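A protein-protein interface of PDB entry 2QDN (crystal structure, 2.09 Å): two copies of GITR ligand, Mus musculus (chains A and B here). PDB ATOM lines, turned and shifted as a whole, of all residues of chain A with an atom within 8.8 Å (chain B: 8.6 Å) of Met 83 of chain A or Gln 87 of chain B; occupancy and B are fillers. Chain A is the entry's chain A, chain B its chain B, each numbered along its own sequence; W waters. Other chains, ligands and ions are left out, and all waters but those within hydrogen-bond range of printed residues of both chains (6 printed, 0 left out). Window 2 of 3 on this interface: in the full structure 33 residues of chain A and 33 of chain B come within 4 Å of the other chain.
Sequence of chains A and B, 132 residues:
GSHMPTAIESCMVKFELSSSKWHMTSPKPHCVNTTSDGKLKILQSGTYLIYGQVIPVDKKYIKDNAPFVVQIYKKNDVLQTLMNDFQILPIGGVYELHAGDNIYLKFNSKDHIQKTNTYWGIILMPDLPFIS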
ATOM      1  N   PRO A  67       4.016  -8.441 -29.942  1.00  0.00           N
ATOM      2  CA  PRO A  67       3.572  -9.483 -29.012  1.00  0.00           C
ATOM      3  C   PRO A  67       2.230 -10.130 -29.382  1.00  0.00           C
ATOM      4  O   PRO A  67       1.372  -9.497 -29.995  1.00  0.00           O
ATOM      5  CB  PRO A  67       3.450  -8.743 -27.670  1.00  0.00           C
ATOM      6  CG  PRO A  67       3.340  -7.310 -28.020  1.00  0.00           C
ATOM      7  CD  PRO A  67       4.119  -7.127 -29.277  1.00  0.00           C
ATOM      8  N   PHE A  68       2.085 -11.385 -28.982  1.00  0.00           N
ATOM      9  CA  PHE A  68       0.827 -12.106 -29.067  1.00  0.00           C
ATOM     10  C   PHE A  68      -0.028 -11.774 -27.840  1.00  0.00           C
ATOM     11  O   PHE A  68       0.226 -12.254 -26.751  1.00  0.00           O
ATOM     12  CB  PHE A  68       1.109 -13.610 -29.160  1.00  0.00           C
ATOM     13  CG  PHE A  68      -0.112 -14.459 -29.136  1.00  0.00           C
ATOM     14  CD1 PHE A  68      -1.175 -14.201 -29.994  1.00  0.00           C
ATOM     15  CD2 PHE A  68      -0.190 -15.556 -28.271  1.00  0.00           C
ATOM     16  CE1 PHE A  68      -2.305 -14.986 -29.969  1.00  0.00           C
ATOM     17  CE2 PHE A  68      -1.306 -16.366 -28.262  1.00  0.00           C
ATOM     18  CZ  PHE A  68      -2.367 -16.088 -29.101  1.00  0.00           C
ATOM     19  N   VAL A  69      -1.044 -10.943 -28.030  1.00  0.00           N
ATOM     20  CA  VAL A  69      -1.889 -10.507 -26.930  1.00  0.00           C
ATOM     21  C   VAL A  69      -3.363 -10.759 -27.261  1.00  0.00           C
ATOM     22  O   VAL A  69      -3.803 -10.502 -28.372  1.00  0.00           O
ATOM     23  CB  VAL A  69      -1.685  -9.017 -26.579  1.00  0.00           C
ATOM     24  CG1 VAL A  69      -2.484  -8.656 -25.301  1.00  0.00           C
ATOM     25  CG2 VAL A  69      -0.172  -8.673 -26.409  1.00  0.00           C
ATOM     26  N   VAL A  70      -4.093 -11.310 -26.288  1.00  0.00           N
ATOM     27  CA  VAL A  70      -5.535 -11.411 -26.397  1.00  0.00           C
ATOM     28  C   VAL A  70      -6.212 -10.709 -25.203  1.00  0.00           C
ATOM     29  O   VAL A  70      -5.914 -11.035 -24.034  1.00  0.00           O
ATOM     30  CB  VAL A  70      -5.998 -12.883 -26.444  1.00  0.00           C
ATOM     31  CG1 VAL A  70      -7.509 -12.957 -26.596  1.00  0.00           C
ATOM     32  CG2 VAL A  70      -5.279 -13.650 -27.575  1.00  0.00           C
ATOM     33  N   GLN A  71      -7.133  -9.795 -25.502  1.00  0.00           N
ATOM     34  CA  GLN A  71      -8.005  -9.193 -24.482  1.00  0.00           C
ATOM     35  C   GLN A  71      -9.464  -9.547 -24.655  1.00  0.00           C
ATOM     36  O   GLN A  71      -9.951  -9.753 -25.768  1.00  0.00           O
ATOM     37  CB  GLN A  71      -7.869  -7.672 -24.465  1.00  0.00           C
ATOM     38  CG  GLN A  71      -6.458  -7.189 -24.124  1.00  0.00           C
ATOM     39  CD  GLN A  71      -6.340  -5.687 -24.195  1.00  0.00           C
ATOM     40  OE1 GLN A  71      -6.660  -5.089 -25.215  1.00  0.00           O
ATOM     41  NE2 GLN A  71      -5.876  -5.063 -23.108  1.00  0.00           N
ATOM     42  N   GLN A  80      -9.891  -8.945 -19.057  1.00  0.00           N
ATOM     43  CA  GLN A  80      -8.590  -9.584 -18.886  1.00  0.00           C
ATOM     44  C   GLN A  80      -7.711  -9.366 -20.115  1.00  0.00           C
ATOM     45  O   GLN A  80      -8.202  -9.151 -21.238  1.00  0.00           O
ATOM     46  CB  GLN A  80      -8.721 -11.102 -18.579  1.00  0.00           C
ATOM     47  CG  GLN A  80      -9.202 -11.940 -19.738  1.00  0.00           C
ATOM     48  CD  GLN A  80      -9.128 -13.463 -19.516  1.00  0.00           C
ATOM     49  OE1 GLN A  80      -8.919 -14.209 -20.468  1.00  0.00           O
ATOM     50  NE2 GLN A  80      -9.308 -13.922 -18.272  1.00  0.00           N
ATOM     51  N   THR A  81      -6.410  -9.426 -19.867  1.00  0.00           N
ATOM     52  CA  THR A  81      -5.382  -9.259 -20.865  1.00  0.00           C
ATOM     53  C   THR A  81      -4.425 -10.415 -20.714  1.00  0.00           C
ATOM     54  O   THR A  81      -3.962 -10.685 -19.623  1.00  0.00           O
ATOM     55  CB  THR A  81      -4.631  -7.947 -20.664  1.00  0.00           C
ATOM     56  OG1 THR A  81      -5.566  -6.864 -20.743  1.00  0.00           O
ATOM     57  CG2 THR A  81      -3.507  -7.792 -21.737  1.00  0.00           C
ATOM     58  N   LEU A  82      -4.165 -11.102 -21.820  1.00  0.00           N
ATOM     59  CA  LEU A  82      -3.369 -12.318 -21.813  1.00  0.00           C
ATOM     60  C   LEU A  82      -2.296 -12.220 -22.881  1.00  0.00           C
ATOM     61  O   LEU A  82      -2.525 -11.662 -23.967  1.00  0.00           O
ATOM     62  CB  LEU A  82      -4.261 -13.538 -22.101  1.00  0.00           C
ATOM     63  CG  LEU A  82      -5.523 -13.734 -21.240  1.00  0.00           C
ATOM     64  CD1 LEU A  82      -6.328 -14.877 -21.815  1.00  0.00           C
ATOM     65  CD2 LEU A  82      -5.233 -13.968 -19.752  1.00  0.00           C
ATOM     66  N   MET A  83      -1.126 -12.760 -22.564  1.00  0.00           N
ATOM     67  CA  MET A  83      -0.033 -12.843 -23.508  1.00  0.00           C
ATOM     68  C   MET A  83       0.850 -14.023 -23.168  1.00  0.00           C
ATOM     69  O   MET A  83       1.082 -14.337 -22.000  1.00  0.00           O
ATOM     70  CB  MET A  83       0.784 -11.537 -23.585  1.00  0.00           C
ATOM     71  CG  MET A  83       0.895 -10.812 -22.282  1.00  0.00           C
ATOM     72  SD  MET A  83       1.742  -9.214 -22.298  1.00  0.00           S
ATOM     73  CE  MET A  83       0.831  -8.386 -20.974  1.00  0.00           C
ATOM     74  N   ASN A  84       1.287 -14.716 -24.206  1.00  0.00           N
ATOM     75  CA  ASN A  84       2.364 -15.698 -24.083  1.00  0.00           C
ATOM     76  C   ASN A  84       3.198 -15.643 -25.374  1.00  0.00           C
ATOM     77  O   ASN A  84       2.938 -14.802 -26.249  1.00  0.00           O
ATOM     78  CB  ASN A  84       1.828 -17.115 -23.729  1.00  0.00           C
ATOM     79  CG  ASN A  84       1.021 -17.730 -24.833  1.00  0.00           C
ATOM     80  OD1 ASN A  84       1.205 -17.407 -26.006  1.00  0.00           O
ATOM     81  ND2 ASN A  84       0.123 -18.621 -24.474  1.00  0.00           N
ATOM     82  N   ASP A  85       4.230 -16.482 -25.461  1.00  0.00           N
ATOM     83  CA  ASP A  85       5.164 -16.462 -26.572  1.00  0.00           C
ATOM     84  C   ASP A  85       4.611 -17.320 -27.698  1.00  0.00           C
ATOM     85  O   ASP A  85       5.195 -18.362 -28.047  1.00  0.00           O
ATOM     86  CB  ASP A  85       6.541 -17.001 -26.126  1.00  0.00           C
ATOM     87  CG  ASP A  85       7.645 -16.718 -27.154  1.00  0.00           C
ATOM     88  OD1 ASP A  85       7.438 -15.878 -28.060  1.00  0.00           O
ATOM     89  OD2 ASP A  85       8.738 -17.339 -27.052  1.00  0.00           O
ATOM     90  N   PHE A  86       3.481 -16.888 -28.262  1.00  0.00           N
ATOM     91  CA  PHE A  86       2.836 -17.609 -29.365  1.00  0.00           C
ATOM     92  C   PHE A  86       2.604 -19.112 -29.105  1.00  0.00           C
ATOM     93  O   PHE A  86       2.967 -19.965 -29.926  1.00  0.00           O
ATOM     94  CB  PHE A  86       3.581 -17.375 -30.680  1.00  0.00           C
ATOM     95  CG  PHE A  86       3.598 -15.920 -31.113  1.00  0.00           C
ATOM     96  CD1 PHE A  86       2.729 -15.469 -32.126  1.00  0.00           C
ATOM     97  CD2 PHE A  86       4.467 -15.012 -30.519  1.00  0.00           C
ATOM     98  CE1 PHE A  86       2.740 -14.139 -32.531  1.00  0.00           C
ATOM     99  CE2 PHE A  86       4.484 -13.692 -30.900  1.00  0.00           C
ATOM    100  CZ  PHE A  86       3.609 -13.237 -31.911  1.00  0.00           C
ATOM    101  N   GLN A  87       1.989 -19.411 -27.964  1.00  0.00           N
ATOM    102  CA  GLN A  87       1.526 -20.755 -27.649  1.00  0.00           C
ATOM    103  C   GLN A  87       0.009 -20.726 -27.465  1.00  0.00           C
ATOM    104  O   GLN A  87      -0.577 -19.670 -27.214  1.00  0.00           O
ATOM    105  CB  GLN A  87       2.219 -21.290 -26.383  1.00  0.00           C
ATOM    106  CG  GLN A  87       3.744 -21.456 -26.509  1.00  0.00           C
ATOM    107  CD  GLN A  87       4.156 -22.456 -27.587  1.00  0.00           C
ATOM    108  OE1 GLN A  87       3.516 -23.482 -27.771  1.00  0.00           O
ATOM    109  NE2 GLN A  87       5.233 -22.156 -28.296  1.00  0.00           N
ATOM    110  N   ILE A  88      -0.614 -21.890 -27.611  1.00  0.00           N
ATOM    111  CA  ILE A  88      -2.066 -22.061 -27.404  1.00  0.00           C
ATOM    112  C   ILE A  88      -2.544 -21.356 -26.112  1.00  0.00           C
ATOM    113  O   ILE A  88      -1.965 -21.549 -25.056  1.00  0.00           O
ATOM    114  CB  ILE A  88      -2.449 -23.561 -27.438  1.00  0.00           C
ATOM    115  CG1 ILE A  88      -2.267 -24.094 -28.869  1.00  0.00           C
ATOM    116  CG2 ILE A  88      -3.896 -23.793 -26.916  1.00  0.00           C
ATOM    117  CD1 ILE A  88      -2.124 -25.656 -28.966  1.00  0.00           C
ATOM    118  N   LEU A  89      -3.571 -20.514 -26.235  1.00  0.00           N
ATOM    119  CA  LEU A  89      -3.989 -19.630 -25.171  1.00  0.00           C
ATOM    120  C   LEU A  89      -5.441 -19.904 -24.753  1.00  0.00           C
ATOM    121  O   LEU A  89      -6.385 -19.456 -25.436  1.00  0.00           O
ATOM    122  CB  LEU A  89      -3.815 -18.161 -25.615  1.00  0.00           C
ATOM    123  CG  LEU A  89      -3.977 -17.055 -24.559  1.00  0.00           C
ATOM    124  CD1 LEU A  89      -2.981 -17.236 -23.420  1.00  0.00           C
ATOM    125  CD2 LEU A  89      -3.774 -15.695 -25.190  1.00  0.00           C
ATOM    126  N   PRO A  90      -5.631 -20.678 -23.653  1.00  0.00           N
ATOM    127  CA  PRO A  90      -6.970 -20.734 -23.088  1.00  0.00           C
ATOM    128  C   PRO A  90      -7.316 -19.361 -22.494  1.00  0.00           C
ATOM    129  O   PRO A  90      -6.432 -18.654 -21.977  1.00  0.00           O
ATOM    130  CB  PRO A  90      -6.873 -21.829 -22.002  1.00  0.00           C
ATOM    131  CG  PRO A  90      -5.552 -22.573 -22.301  1.00  0.00           C
ATOM    132  CD  PRO A  90      -4.672 -21.507 -22.896  1.00  0.00           C
ATOM    133  N   ILE A  91      -8.584 -18.984 -22.588  1.00  0.00           N
ATOM    134  CA  ILE A  91      -9.012 -17.640 -22.176  1.00  0.00           C
ATOM    135  C   ILE A  91     -10.215 -17.747 -21.246  1.00  0.00           C
ATOM    136  O   ILE A  91     -10.861 -18.786 -21.199  1.00  0.00           O
ATOM    137  CB  ILE A  91      -9.421 -16.739 -23.396  1.00  0.00           C
ATOM    138  CG1 ILE A  91     -10.806 -17.149 -23.950  1.00  0.00           C
ATOM    139  CG2 ILE A  91      -8.307 -16.716 -24.508  1.00  0.00           C
ATOM    140  CD1 ILE A  91     -11.292 -16.295 -25.184  1.00  0.00           C
ATOM    141  N   ASN A 108      -3.926  -8.141 -30.362  1.00  0.00           N
ATOM    142  CA  ASN A 108      -2.872  -7.195 -30.761  1.00  0.00           C
ATOM    143  C   ASN A 108      -2.698  -7.126 -32.285  1.00  0.00           C
ATOM    144  O   ASN A 108      -2.577  -6.020 -32.852  1.00  0.00           O
ATOM    145  CB  ASN A 108      -1.527  -7.484 -30.094  1.00  0.00           C
ATOM    146  CG  ASN A 108      -0.505  -6.370 -30.340  1.00  0.00           C
ATOM    147  OD1 ASN A 108      -0.832  -5.174 -30.287  1.00  0.00           O
ATOM    148  ND2 ASN A 108       0.721  -6.754 -30.628  1.00  0.00           N
ATOM    149  N   GLN B  53      -8.827 -20.256 -13.183  1.00  0.00           N
ATOM    150  CA  GLN B  53      -7.780 -19.257 -13.298  1.00  0.00           C
ATOM    151  C   GLN B  53      -6.762 -19.538 -12.225  1.00  0.00           C
ATOM    152  O   GLN B  53      -7.129 -19.706 -11.057  1.00  0.00           O
ATOM    153  CB  GLN B  53      -8.326 -17.843 -13.144  1.00  0.00           C
ATOM    154  CG  GLN B  53      -9.175 -17.365 -14.290  1.00  0.00           C
ATOM    155  CD  GLN B  53      -9.579 -15.927 -14.146  1.00  0.00           C
ATOM    156  OE1 GLN B  53      -9.359 -15.314 -13.101  1.00  0.00           O
ATOM    157  NE2 GLN B  53     -10.177 -15.369 -15.201  1.00  0.00           N
ATOM    158  N   VAL B  54      -5.498 -19.620 -12.631  1.00  0.00           N
ATOM    159  CA  VAL B  54      -4.372 -19.712 -11.700  1.00  0.00           C
ATOM    160  C   VAL B  54      -3.677 -18.336 -11.591  1.00  0.00           C
ATOM    161  O   VAL B  54      -3.207 -17.779 -12.580  1.00  0.00           O
ATOM    162  CB  VAL B  54      -3.406 -20.840 -12.127  1.00  0.00           C
ATOM    163  CG1 VAL B  54      -2.240 -20.974 -11.145  1.00  0.00           C
ATOM    164  CG2 VAL B  54      -4.174 -22.165 -12.278  1.00  0.00           C
ATOM    165  N   ILE B  55      -3.696 -17.753 -10.399  1.00  0.00           N
ATOM    166  CA  ILE B  55      -3.158 -16.410 -10.216  1.00  0.00           C
ATOM    167  C   ILE B  55      -1.783 -16.528  -9.565  1.00  0.00           C
ATOM    168  O   ILE B  55      -1.674 -17.082  -8.487  1.00  0.00           O
ATOM    169  CB  ILE B  55      -4.104 -15.475  -9.374  1.00  0.00           C
ATOM    170  CG1 ILE B  55      -5.553 -15.514  -9.908  1.00  0.00           C
ATOM    171  CG2 ILE B  55      -3.568 -14.032  -9.342  1.00  0.00           C
ATOM    172  CD1 ILE B  55      -5.730 -15.120 -11.356  1.00  0.00           C
ATOM    173  N   PRO B  56      -0.725 -16.045 -10.251  1.00  0.00           N
ATOM    174  CA  PRO B  56       0.617 -16.086  -9.651  1.00  0.00           C
ATOM    175  C   PRO B  56       0.808 -15.002  -8.604  1.00  0.00           C
ATOM    176  O   PRO B  56       0.167 -13.956  -8.689  1.00  0.00           O
ATOM    177  CB  PRO B  56       1.549 -15.821 -10.836  1.00  0.00           C
ATOM    178  CG  PRO B  56       0.720 -14.993 -11.792  1.00  0.00           C
ATOM    179  CD  PRO B  56      -0.732 -15.425 -11.591  1.00  0.00           C
ATOM    180  N   VAL B  57       1.668 -15.262  -7.617  1.00  0.00           N
ATOM    181  CA  VAL B  57       2.136 -14.211  -6.716  1.00  0.00           C
ATOM    182  C   VAL B  57       3.043 -13.258  -7.509  1.00  0.00           C
ATOM    183  O   VAL B  57       3.574 -13.632  -8.545  1.00  0.00           O
ATOM    184  CB  VAL B  57       2.867 -14.776  -5.460  1.00  0.00           C
ATOM    185  CG1 VAL B  57       1.897 -15.603  -4.579  1.00  0.00           C
ATOM    186  CG2 VAL B  57       4.085 -15.590  -5.851  1.00  0.00           C
ATOM    187  N   ASP B  58       3.166 -12.016  -7.051  1.00  0.00           N
ATOM    188  CA  ASP B  58       4.098 -11.047  -7.624  1.00  0.00           C
ATOM    189  C   ASP B  58       5.506 -11.661  -7.637  1.00  0.00           C
ATOM    190  O   ASP B  58       5.919 -12.320  -6.665  1.00  0.00           O
ATOM    191  CB  ASP B  58       4.055  -9.762  -6.781  1.00  0.00           C
ATOM    192  CG  ASP B  58       4.836  -8.599  -7.398  1.00  0.00           C
ATOM    193  OD1 ASP B  58       5.999  -8.785  -7.834  1.00  0.00           O
ATOM    194  OD2 ASP B  58       4.290  -7.467  -7.397  1.00  0.00           O
ATOM    195  N   LYS B  59       6.222 -11.475  -8.754  1.00  0.00           N
ATOM    196  CA  LYS B  59       7.594 -11.995  -8.900  1.00  0.00           C
ATOM    197  C   LYS B  59       8.558 -11.526  -7.799  1.00  0.00           C
ATOM    198  O   LYS B  59       9.505 -12.218  -7.492  1.00  0.00           O
ATOM    199  CB  LYS B  59       8.171 -11.681 -10.285  1.00  0.00           C
ATOM    200  CG  LYS B  59       7.636 -12.568 -11.422  1.00  0.00           C
ATOM    201  CD  LYS B  59       8.244 -12.170 -12.793  1.00  0.00           C
ATOM    202  CE  LYS B  59       9.670 -12.705 -12.945  1.00  0.00           C
ATOM    203  NZ  LYS B  59      10.275 -12.442 -14.296  1.00  0.00           N
ATOM    204  N   PHE B  68       7.112 -20.696 -13.920  1.00  0.00           N
ATOM    205  CA  PHE B  68       5.659 -20.748 -13.690  1.00  0.00           C
ATOM    206  C   PHE B  68       5.004 -21.679 -14.704  1.00  0.00           C
ATOM    207  O   PHE B  68       4.831 -21.325 -15.883  1.00  0.00           O
ATOM    208  CB  PHE B  68       5.052 -19.336 -13.781  1.00  0.00           C
ATOM    209  CG  PHE B  68       3.578 -19.247 -13.373  1.00  0.00           C
ATOM    210  CD1 PHE B  68       3.145 -19.700 -12.126  1.00  0.00           C
ATOM    211  CD2 PHE B  68       2.642 -18.659 -14.231  1.00  0.00           C
ATOM    212  CE1 PHE B  68       1.781 -19.590 -11.746  1.00  0.00           C
ATOM    213  CE2 PHE B  68       1.289 -18.541 -13.868  1.00  0.00           C
ATOM    214  CZ  PHE B  68       0.857 -19.009 -12.624  1.00  0.00           C
ATOM    215  N   VAL B  70       1.829 -24.672 -15.200  1.00  0.00           N
ATOM    216  CA  VAL B  70       0.643 -25.372 -14.730  1.00  0.00           C
ATOM    217  C   VAL B  70       0.340 -26.500 -15.712  1.00  0.00           C
ATOM    218  O   VAL B  70       0.328 -26.278 -16.919  1.00  0.00           O
ATOM    219  CB  VAL B  70      -0.578 -24.415 -14.617  1.00  0.00           C
ATOM    220  CG1 VAL B  70      -1.815 -25.168 -14.143  1.00  0.00           C
ATOM    221  CG2 VAL B  70      -0.269 -23.225 -13.694  1.00  0.00           C
ATOM    222  N   MET B  83       2.134 -22.235 -19.497  1.00  0.00           N
ATOM    223  CA  MET B  83       3.259 -21.501 -18.945  1.00  0.00           C
ATOM    224  C   MET B  83       3.283 -20.070 -19.434  1.00  0.00           C
ATOM    225  O   MET B  83       2.954 -19.780 -20.585  1.00  0.00           O
ATOM    226  CB  MET B  83       4.604 -22.213 -19.236  1.00  0.00           C
ATOM    227  CG  MET B  83       4.980 -22.342 -20.713  1.00  0.00           C
ATOM    228  SD  MET B  83       6.443 -23.399 -21.087  1.00  0.00           S
ATOM    229  CE  MET B  83       5.879 -25.059 -20.720  1.00  0.00           C
ATOM    230  N   ASN B  84       3.664 -19.174 -18.546  1.00  0.00           N
ATOM    231  CA  ASN B  84       3.907 -17.784 -18.904  1.00  0.00           C
ATOM    232  C   ASN B  84       4.842 -17.177 -17.851  1.00  0.00           C
ATOM    233  O   ASN B  84       5.302 -17.883 -16.949  1.00  0.00           O
ATOM    234  CB  ASN B  84       2.587 -16.996 -19.100  1.00  0.00           C
ATOM    235  CG  ASN B  84       1.816 -16.756 -17.787  1.00  0.00           C
ATOM    236  OD1 ASN B  84       2.384 -16.803 -16.697  1.00  0.00           O
ATOM    237  ND2 ASN B  84       0.519 -16.469 -17.907  1.00  0.00           N
ATOM    238  N   ASP B  85       5.133 -15.885 -17.985  1.00  0.00           N
ATOM    239  CA  ASP B  85       6.064 -15.177 -17.107  1.00  0.00           C
ATOM    240  C   ASP B  85       5.341 -14.657 -15.849  1.00  0.00           C
ATOM    241  O   ASP B  85       5.256 -13.446 -15.625  1.00  0.00           O
ATOM    242  CB  ASP B  85       6.684 -14.013 -17.909  1.00  0.00           C
ATOM    243  CG  ASP B  85       7.820 -13.339 -17.195  1.00  0.00           C
ATOM    244  OD1 ASP B  85       8.484 -13.988 -16.347  1.00  0.00           O
ATOM    245  OD2 ASP B  85       8.053 -12.144 -17.502  1.00  0.00           O
ATOM    246  N   PHE B  86       4.812 -15.574 -15.042  1.00  0.00           N
ATOM    247  CA  PHE B  86       4.092 -15.221 -13.805  1.00  0.00           C
ATOM    248  C   PHE B  86       2.988 -14.190 -14.017  1.00  0.00           C
ATOM    249  O   PHE B  86       2.982 -13.126 -13.388  1.00  0.00           O
ATOM    250  CB  PHE B  86       5.070 -14.766 -12.712  1.00  0.00           C
ATOM    251  CG  PHE B  86       6.040 -15.836 -12.302  1.00  0.00           C
ATOM    252  CD1 PHE B  86       5.789 -16.623 -11.191  1.00  0.00           C
ATOM    253  CD2 PHE B  86       7.199 -16.074 -13.052  1.00  0.00           C
ATOM    254  CE1 PHE B  86       6.655 -17.630 -10.830  1.00  0.00           C
ATOM    255  CE2 PHE B  86       8.084 -17.073 -12.664  1.00  0.00           C
ATOM    256  CZ  PHE B  86       7.808 -17.842 -11.564  1.00  0.00           C
ATOM    257  N   GLN B  87       2.056 -14.531 -14.910  1.00  0.00           N
ATOM    258  CA  GLN B  87       0.912 -13.691 -15.218  1.00  0.00           C
ATOM    259  C   GLN B  87      -0.355 -14.525 -15.089  1.00  0.00           C
ATOM    260  O   GLN B  87      -0.293 -15.770 -15.091  1.00  0.00           O
ATOM    261  CB  GLN B  87       1.013 -13.162 -16.644  1.00  0.00           C
ATOM    262  CG  GLN B  87       2.139 -12.224 -16.884  1.00  0.00           C
ATOM    263  CD  GLN B  87       2.055 -11.562 -18.261  1.00  0.00           C
ATOM    264  OE1 GLN B  87       2.640 -10.501 -18.473  1.00  0.00           O
ATOM    265  NE2 GLN B  87       1.334 -12.192 -19.200  1.00  0.00           N
ATOM    266  N   ILE B  88      -1.490 -13.839 -14.979  1.00  0.00           N
ATOM    267  CA  ILE B  88      -2.793 -14.488 -14.874  1.00  0.00           C
ATOM    268  C   ILE B  88      -2.899 -15.629 -15.895  1.00  0.00           C
ATOM    269  O   ILE B  88      -2.606 -15.446 -17.090  1.00  0.00           O
ATOM    270  CB  ILE B  88      -3.961 -13.463 -15.041  1.00  0.00           C
ATOM    271  CG1 ILE B  88      -5.326 -14.169 -14.980  1.00  0.00           C
ATOM    272  CG2 ILE B  88      -3.807 -12.628 -16.353  1.00  0.00           C
ATOM    273  CD1 ILE B  88      -6.525 -13.227 -15.230  1.00  0.00           C
ATOM    274  N   LEU B  89      -3.305 -16.807 -15.418  1.00  0.00           N
ATOM    275  CA  LEU B  89      -3.408 -17.970 -16.303  1.00  0.00           C
ATOM    276  C   LEU B  89      -4.769 -18.687 -16.248  1.00  0.00           C
ATOM    277  O   LEU B  89      -4.983 -19.570 -15.393  1.00  0.00           O
ATOM    278  CB  LEU B  89      -2.265 -18.942 -16.025  1.00  0.00           C
ATOM    279  CG  LEU B  89      -1.960 -20.034 -17.042  1.00  0.00           C
ATOM    280  CD1 LEU B  89      -1.086 -19.568 -18.286  1.00  0.00           C
ATOM    281  CD2 LEU B  89      -1.228 -21.079 -16.240  1.00  0.00           C
ATOM    282  N   PRO B  90      -5.686 -18.324 -17.178  1.00  0.00           N
ATOM    283  CA  PRO B  90      -6.874 -19.163 -17.439  1.00  0.00           C
ATOM    284  C   PRO B  90      -6.420 -20.489 -18.020  1.00  0.00           C
ATOM    285  O   PRO B  90      -5.397 -20.551 -18.712  1.00  0.00           O
ATOM    286  CB  PRO B  90      -7.692 -18.355 -18.465  1.00  0.00           C
ATOM    287  CG  PRO B  90      -7.128 -16.924 -18.379  1.00  0.00           C
ATOM    288  CD  PRO B  90      -5.665 -17.112 -18.016  1.00  0.00           C
ATOM    289  N   HIS B 112       4.344 -20.460  -5.964  1.00  0.00           N
ATOM    290  CA  HIS B 112       4.032 -19.522  -7.069  1.00  0.00           C
ATOM    291  C   HIS B 112       2.598 -18.996  -7.055  1.00  0.00           C
ATOM    292  O   HIS B 112       2.283 -17.963  -7.675  1.00  0.00           O
ATOM    293  CB  HIS B 112       4.273 -20.189  -8.429  1.00  0.00           C
ATOM    294  CG  HIS B 112       5.711 -20.504  -8.708  1.00  0.00           C
ATOM    295  ND1 HIS B 112       6.106 -21.270  -9.786  1.00  0.00           N
ATOM    296  CD2 HIS B 112       6.846 -20.148  -8.061  1.00  0.00           C
ATOM    297  CE1 HIS B 112       7.425 -21.371  -9.790  1.00  0.00           C
ATOM    298  NE2 HIS B 112       7.898 -20.704  -8.751  1.00  0.00           N
HETATM  299  O   HOH W   1       3.771 -13.958 -20.132  1.00  0.00           O
HETATM  300  O   HOH W   2       4.829 -18.771 -23.357  1.00  0.00           O
HETATM  301  O   HOH W   3      -4.121 -18.975 -20.616  1.00  0.00           O
HETATM  302  O   HOH W   4      -0.321 -16.612 -20.561  1.00  0.00           O
HETATM  303  O   HOH W   5      -1.133 -13.730 -19.493  1.00  0.00           O
HETATM  304  O   HOH W   6      -1.383 -10.598 -18.883  1.00  0.00           O
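Val 70 of chain A touches none of the printed residues of chain B. Printed residues of chain B within 4 Å of Gln 80 of chain A: Gln 53 and Pro 90. Met 83 of chain A touches just one residue of chain B: Gln 87. Printed residues of chain B within 4 Å of Pro 90 of chain A: Pro 90. Of the printed residues of chain B, Ile 91 of chain A touches Pro 90. Pro 56 of chain B touches none of the printed residues of chain A. Of chain A, only Met 83 comes within 4 Å of Gln 87 of chain B. Of the printed residues of chain A, Pro 90 of chain B touches Gln 80 (3.7 Å), Leu 82 (3.6 Å), Pro 90 (3.7 Å) and Ile 91 (3.8 Å). The nearest residue of chain B that does not touch Met 83 of chain A is Asn 84 of chain B (4.2 Å). The nearest printed residue of chain A that does not touch Pro 90 of chain B is Leu 89 of chain A (6.0 Å).
Among the printed residues, pairs that only touch across the chains: Gln 80 of chain A with Gln 53 of chain B, Gln 80 of chain A with Pro 90 of chain B, Thr 81 of chain A with Ile 88 of chain B, Leu 82 of chain A with Ile 88 of chain B, Leu 82 of chain A with Pro 90 of chain B, Met 83 of chain A with Gln 87 of chain B, Pro 90 of chain A with Pro 90 of chain B and Ile 91 of chain A with Pro 90 of chain B.
Water W3 lies within hydrogen-bond range of the backbone carbonyl oxygen (O) of Pro 90 of chain A (2.7 Å) and the backbone carbonyl oxygen (O) of Pro 90 of chain B (2.8 Å). Water W4 lies within hydrogen-bond range of the side-chain amide nitrogen of Asn 84 of chain B (2.8 Å) and the backbone carbonyl oxygen of Met 83 of chain A (3.0 Å).
Of the 18 printed residues of chain B, 4 touch a printed residue of chain A. Printed residues of chain B that touch a printed residue of chain A: Gln 53, Gln 87, Ile 88 and Pro 90. Hydrophobic or aromatic side chains of chain B that line the printed part of chain A: Ile 88 and Pro 90. Of the 18 printed residues of chain A, 6 touch a printed residue of chain B. Hydrophobic or aromatic side chains of chain A that line the printed part of chain B: Leu 82, Met 83 and Pro 90. Along chain A the printed residues that touch a printed residue of chain B span positions 80 to 91. Among the printed residues, no Asp or Glu carboxylate lies within 4 Å of a Lys or Arg side-chain nitrogen of the other chain.
Met 83 of chain A touches Gln 87 of chain B, but with the chains exchanged Gln 87 of chain A does not touch Met 83 of chain B (6.0 Å). Pro 90 of chain A touches its own counterpart, Pro 90 of chain B. Positions printed for both chains: 68, 70, 83, 84, 85, 86, 87, 88, 89 and 90. Of the 8 pairs that touch across the chains among the printed residues, 1 has its exchanged pair printed and touching as well.
The side-chain amide nitrogen (NE2) of Gln 71 of chain A lies within hydrogen-bond range of the side-chain hydroxyl (OG1) of Thr 81 of chain A (3.0 Å). The side-chain amide nitrogen of Asn 84 of chain B lies within hydrogen-bond range of the backbone carbonyl oxygen of Ile 88 of chain B (3.4 Å). N of Leu 82 of chain A lies within hydrogen-bond range of O of Val 70 of chain A (2.8 Å).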
